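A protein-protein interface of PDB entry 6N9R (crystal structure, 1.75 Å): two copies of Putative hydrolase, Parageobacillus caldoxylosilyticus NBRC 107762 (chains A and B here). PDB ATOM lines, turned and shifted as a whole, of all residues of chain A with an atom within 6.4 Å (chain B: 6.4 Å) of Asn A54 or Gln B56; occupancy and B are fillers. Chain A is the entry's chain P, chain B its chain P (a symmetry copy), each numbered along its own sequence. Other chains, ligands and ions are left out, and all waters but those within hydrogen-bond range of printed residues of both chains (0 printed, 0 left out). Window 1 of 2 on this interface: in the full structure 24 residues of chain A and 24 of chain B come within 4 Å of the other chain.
N of Phe B59 lies within hydrogen-bond range of O of Pro A53 (3.3 Å).
OD1 of Asn A54 sits close to O of Thr B57 (3.4 Å).
The backbone carbonyl oxygen (O) of Ala A55 sits at hydrogen-bond distance from the backbone NH (N) of Thr B57 (3.1 Å).
O of Thr A57 sits close to OD1 of Asn B54 (3.4 Å).
O of Ala B55 is in hydrogen-bond range of N of Thr A57.
The backbone NH (N) of Asn A52 is in hydrogen-bond range of the side-chain hydroxyl (OG1) of Thr A49 (3.1 Å).
A ring nitrogen (NE2) of His B45 is in hydrogen-bond range of the side-chain hydroxyl (OG1) of Thr B57, at 3.2 Å.
The side-chain amide nitrogen (ND2) of Asn B46 is in hydrogen-bond range of the backbone carbonyl oxygen (O) of Gln B56, at 3.2 Å.
Among the printed residues, pairs that only touch across the chains: Ala A48 with Thr B57, Ala A48 with Phe B59, Thr A49 with Phe B59, Pro A53 with Glu B58, Asn A54 with Gln B56, Ala A55 with Gln B56, Gln A56 with Asn B54, Gln A56 with Ala B55 and Gln A56 with Gln B56.
Of the printed residues of chain B, Thr A49 touches Phe B59 (3.7 Å).
Of the printed residues of chain B, Pro A53 touches Glu B58 (3.4 Å) and Phe B59 (3.3 Å).
Of the printed residues of chain B, Asn A54 touches Gln B56 (3.3 Å) and Thr B57 (3.4 Å).
Of the printed residues of chain B, Gln A56 touches Asn B54 (3.3 Å), Ala B55 (3.5 Å) and Gln B56 (3.3 Å).
His B45 touches none of the printed residues of chain A.
Asn B46 touches none of the printed residues of chain A.
Of the printed residues of chain A, Thr B57 touches Ala A48, Asn A54 and Ala A55.
Of the printed residues of chain A, Phe B59 touches Ala A48 (3.6 Å), Thr A49 (3.7 Å) and Pro A53 (3.3 Å).
The nearest printed residue of chain B that does not touch Asn A54 is Glu B58 (4.02 Å).
The nearest residue of chain A that does not touch Gln B56 is Thr A57 (5.2 Å).
Along chain B the printed residues that touch a printed residue of chain A span positions 54 to 59.
Of the 8 printed residues of chain A, 7 touch a printed residue of chain B.
Hydrophobic or aromatic side chains of chain A within 4 Å of the printed part of chain B: Ala A48 and Pro A53.
Among the printed residues, 14 pairs touch across the chains.
Among the printed residues, no Asp or Glu carboxylate lies within 4 Å of a Lys or Arg side-chain nitrogen of the other chain.
Asn A54 touches Gln B56, and with the chains exchanged Gln A56 touches Asn B54.
Asn A54 touches Thr B57, and with the chains exchanged Thr A57 touches Asn B54.
Ala A55 touches Thr B57, and with the chains exchanged Thr A57 touches Ala B55.
Gln A56 touches its own counterpart, Gln B56.
Of the 14 pairs that touch across the chains among the printed residues, 9 have their exchanged pair printed and touching as well.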
ATOM      1  N   ALA A  48      20.866 -25.450   6.028  1.00  0.00           N
ATOM      2  CA  ALA A  48      20.641 -24.018   5.938  1.00  0.00           C
ATOM      3  C   ALA A  48      19.132 -23.747   5.910  1.00  0.00           C
ATOM      4  O   ALA A  48      18.361 -24.546   5.380  1.00  0.00           O
ATOM      5  CB  ALA A  48      21.325 -23.465   4.711  1.00  0.00           C
ATOM      6  N   THR A  49      18.731 -22.616   6.498  1.00  0.00           N
ATOM      7  CA  THR A  49      17.344 -22.165   6.497  1.00  0.00           C
ATOM      8  C   THR A  49      17.291 -20.699   6.057  1.00  0.00           C
ATOM      9  O   THR A  49      18.326 -20.071   5.832  1.00  0.00           O
ATOM     10  CB  THR A  49      16.696 -22.352   7.875  1.00  0.00           C
ATOM     11  OG1 THR A  49      17.386 -21.518   8.807  1.00  0.00           O
ATOM     12  CG2 THR A  49      16.725 -23.789   8.351  1.00  0.00           C
ATOM     13  N   ASN A  52      19.004 -18.910   8.538  1.00  0.00           N
ATOM     14  CA  ASN A  52      20.406 -19.331   8.662  1.00  0.00           C
ATOM     15  C   ASN A  52      20.882 -19.850   7.308  1.00  0.00           C
ATOM     16  O   ASN A  52      21.182 -21.033   7.159  1.00  0.00           O
ATOM     17  CB  ASN A  52      20.599 -20.378   9.763  1.00  0.00           C
ATOM     18  CG  ASN A  52      22.053 -20.602  10.127  1.00  0.00           C
ATOM     19  OD1 ASN A  52      22.908 -19.773   9.824  1.00  0.00           O
ATOM     20  ND2 ASN A  52      22.342 -21.715  10.781  1.00  0.00           N
ATOM     21  N   PRO A  53      20.965 -18.974   6.281  1.00  0.00           N
ATOM     22  CA  PRO A  53      21.290 -19.399   4.916  1.00  0.00           C
ATOM     23  C   PRO A  53      22.749 -19.826   4.693  1.00  0.00           C
ATOM     24  O   PRO A  53      23.058 -20.457   3.681  1.00  0.00           O
ATOM     25  CB  PRO A  53      20.998 -18.135   4.092  1.00  0.00           C
ATOM     26  CG  PRO A  53      21.263 -17.004   5.061  1.00  0.00           C
ATOM     27  CD  PRO A  53      20.735 -17.524   6.382  1.00  0.00           C
ATOM     28  N   ASN A  54      23.630 -19.467   5.632  1.00  0.00           N
ATOM     29  CA  ASN A  54      25.051 -19.783   5.533  1.00  0.00           C
ATOM     30  C   ASN A  54      25.441 -20.683   6.709  1.00  0.00           C
ATOM     31  O   ASN A  54      26.544 -20.580   7.249  1.00  0.00           O
ATOM     32  CB  ASN A  54      25.904 -18.514   5.474  1.00  0.00           C
ATOM     33  CG  ASN A  54      25.595 -17.662   4.261  1.00  0.00           C
ATOM     34  OD1 ASN A  54      25.642 -18.141   3.131  1.00  0.00           O
ATOM     35  ND2 ASN A  54      25.278 -16.397   4.486  1.00  0.00           N
ATOM     36  N   ALA A  55      24.511 -21.567   7.085  1.00  0.00           N
ATOM     37  CA  ALA A  55      24.678 -22.484   8.203  1.00  0.00           C
ATOM     38  C   ALA A  55      26.106 -23.039   8.208  1.00  0.00           C
ATOM     39  O   ALA A  55      26.639 -23.428   7.169  1.00  0.00           O
ATOM     40  CB  ALA A  55      23.658 -23.592   8.114  1.00  0.00           C
ATOM     41  N   GLN A  56      26.708 -23.069   9.401  1.00  0.00           N
ATOM     42  CA  GLN A  56      28.054 -23.580   9.596  1.00  0.00           C
ATOM     43  C   GLN A  56      27.979 -25.045  10.040  1.00  0.00           C
ATOM     44  O   GLN A  56      27.089 -25.432  10.799  1.00  0.00           O
ATOM     45  CB  GLN A  56      28.803 -22.743  10.634  1.00  0.00           C
ATOM     46  CG  GLN A  56      29.248 -21.384  10.115  1.00  0.00           C
ATOM     47  CD  GLN A  56      29.868 -20.533  11.196  1.00  0.00           C
ATOM     48  OE1 GLN A  56      30.609 -21.016  12.050  1.00  0.00           O
ATOM     49  NE2 GLN A  56      29.567 -19.245  11.164  1.00  0.00           N
ATOM     50  N   THR A  57      28.927 -25.847   9.549  1.00  0.00           N
ATOM     51  CA  THR A  57      29.104 -27.216  10.004  1.00  0.00           C
ATOM     52  C   THR A  57      30.048 -27.199  11.211  1.00  0.00           C
ATOM     53  O   THR A  57      30.358 -26.134  11.747  1.00  0.00           O
ATOM     54  CB  THR A  57      29.617 -28.114   8.872  1.00  0.00           C
ATOM     55  OG1 THR A  57      29.554 -29.470   9.318  1.00  0.00           O
ATOM     56  CG2 THR A  57      31.029 -27.779   8.445  1.00  0.00           C
ATOM     57  N   HIS B  45      29.460 -30.391  -0.894  1.00  0.00           N
ATOM     58  CA  HIS B  45      29.942 -29.503  -1.949  1.00  0.00           C
ATOM     59  C   HIS B  45      31.135 -28.677  -1.452  1.00  0.00           C
ATOM     60  O   HIS B  45      31.940 -28.204  -2.253  1.00  0.00           O
ATOM     61  CB  HIS B  45      28.804 -28.606  -2.459  1.00  0.00           C
ATOM     62  CG  HIS B  45      28.451 -27.494  -1.531  1.00  0.00           C
ATOM     63  ND1 HIS B  45      28.939 -26.211  -1.695  1.00  0.00           N
ATOM     64  CD2 HIS B  45      27.666 -27.463  -0.432  1.00  0.00           C
ATOM     65  CE1 HIS B  45      28.467 -25.438  -0.738  1.00  0.00           C
ATOM     66  NE2 HIS B  45      27.684 -26.183   0.050  1.00  0.00           N
ATOM     67  N   ASN B  46      31.236 -28.504  -0.131  1.00  0.00           N
ATOM     68  CA  ASN B  46      32.276 -27.669   0.471  1.00  0.00           C
ATOM     69  C   ASN B  46      32.619 -28.202   1.859  1.00  0.00           C
ATOM     70  O   ASN B  46      32.283 -27.582   2.866  1.00  0.00           O
ATOM     71  CB  ASN B  46      31.845 -26.201   0.538  1.00  0.00           C
ATOM     72  CG  ASN B  46      32.907 -25.300   1.133  1.00  0.00           C
ATOM     73  OD1 ASN B  46      34.092 -25.456   0.848  1.00  0.00           O
ATOM     74  ND2 ASN B  46      32.491 -24.353   1.959  1.00  0.00           N
ATOM     75  N   ASN B  52      39.442 -24.743   7.774  1.00  0.00           N
ATOM     76  CA  ASN B  52      38.066 -24.234   7.688  1.00  0.00           C
ATOM     77  C   ASN B  52      37.135 -25.223   8.384  1.00  0.00           C
ATOM     78  O   ASN B  52      36.291 -25.846   7.744  1.00  0.00           O
ATOM     79  CB  ASN B  52      37.634 -23.980   6.240  1.00  0.00           C
ATOM     80  CG  ASN B  52      36.356 -23.173   6.131  1.00  0.00           C
ATOM     81  OD1 ASN B  52      35.950 -22.512   7.084  1.00  0.00           O
ATOM     82  ND2 ASN B  52      35.719 -23.215   4.973  1.00  0.00           N
ATOM     83  N   ASN B  54      34.613 -24.857  10.387  1.00  0.00           N
ATOM     84  CA  ASN B  54      33.226 -24.432  10.533  1.00  0.00           C
ATOM     85  C   ASN B  54      32.708 -23.952   9.174  1.00  0.00           C
ATOM     86  O   ASN B  54      31.922 -23.007   9.091  1.00  0.00           O
ATOM     87  CB  ASN B  54      33.078 -23.359  11.615  1.00  0.00           C
ATOM     88  CG  ASN B  54      33.496 -23.853  12.983  1.00  0.00           C
ATOM     89  OD1 ASN B  54      32.998 -24.870  13.461  1.00  0.00           O
ATOM     90  ND2 ASN B  54      34.409 -23.140  13.622  1.00  0.00           N
ATOM     91  N   ALA B  55      33.167 -24.629   8.116  1.00  0.00           N
ATOM     92  CA  ALA B  55      32.822 -24.303   6.741  1.00  0.00           C
ATOM     93  C   ALA B  55      31.337 -23.938   6.652  1.00  0.00           C
ATOM     94  O   ALA B  55      30.483 -24.613   7.227  1.00  0.00           O
ATOM     95  CB  ALA B  55      33.157 -25.465   5.839  1.00  0.00           C
ATOM     96  N   GLN B  56      31.052 -22.859   5.917  1.00  0.00           N
ATOM     97  CA  GLN B  56      29.696 -22.380   5.709  1.00  0.00           C
ATOM     98  C   GLN B  56      29.162 -22.933   4.384  1.00  0.00           C
ATOM     99  O   GLN B  56      29.899 -23.052   3.404  1.00  0.00           O
ATOM    100  CB  GLN B  56      29.661 -20.850   5.704  1.00  0.00           C
ATOM    101  CG  GLN B  56      29.812 -20.232   7.086  1.00  0.00           C
ATOM    102  CD  GLN B  56      29.904 -18.726   7.033  1.00  0.00           C
ATOM    103  OE1 GLN B  56      29.216 -18.067   6.257  1.00  0.00           O
ATOM    104  NE2 GLN B  56      30.761 -18.168   7.871  1.00  0.00           N
ATOM    105  N   THR B  57      27.870 -23.270   4.377  1.00  0.00           N
ATOM    106  CA  THR B  57      27.167 -23.645   3.161  1.00  0.00           C
ATOM    107  C   THR B  57      26.613 -22.369   2.519  1.00  0.00           C
ATOM    108  O   THR B  57      26.959 -21.260   2.931  1.00  0.00           O
ATOM    109  CB  THR B  57      26.071 -24.678   3.450  1.00  0.00           C
ATOM    110  OG1 THR B  57      25.579 -25.164   2.201  1.00  0.00           O
ATOM    111  CG2 THR B  57      24.930 -24.116   4.269  1.00  0.00           C
ATOM    112  N   GLU B  58      25.757 -22.537   1.508  1.00  0.00           N
ATOM    113  CA  GLU B  58      25.084 -21.415   0.867  1.00  0.00           C
ATOM    114  C   GLU B  58      23.634 -21.803   0.564  1.00  0.00           C
ATOM    115  O   GLU B  58      23.299 -22.984   0.470  1.00  0.00           O
ATOM    116  CB  GLU B  58      25.838 -20.975  -0.391  1.00  0.00           C
ATOM    117  CG  GLU B  58      26.331 -22.128  -1.249  1.00  0.00           C
ATOM    118  CD  GLU B  58      27.118 -21.702  -2.478  1.00  0.00           C
ATOM    119  OE1 GLU B  58      26.991 -20.528  -2.880  1.00  0.00           O
ATOM    120  OE2 GLU B  58      27.857 -22.543  -3.028  1.00  0.00           O
ATOM    121  N   PHE B  59      22.786 -20.779   0.433  1.00  0.00           N
ATOM    122  CA  PHE B  59      21.352 -20.919   0.206  1.00  0.00           C
ATOM    123  C   PHE B  59      21.057 -20.537  -1.252  1.00  0.00           C
ATOM    124  O   PHE B  59      20.882 -19.361  -1.566  1.00  0.00           O
ATOM    125  CB  PHE B  59      20.599 -20.039   1.209  1.00  0.00           C
ATOM    126  CG  PHE B  59      19.240 -20.533   1.640  1.00  0.00           C
ATOM    127  CD1 PHE B  59      19.084 -21.780   2.223  1.00  0.00           C
ATOM    128  CD2 PHE B  59      18.121 -19.725   1.506  1.00  0.00           C
ATOM    129  CE1 PHE B  59      17.835 -22.221   2.632  1.00  0.00           C
ATOM    130  CE2 PHE B  59      16.874 -20.166   1.919  1.00  0.00           C
ATOM    131  CZ  PHE B  59      16.732 -21.412   2.481  1.00  0.00           C
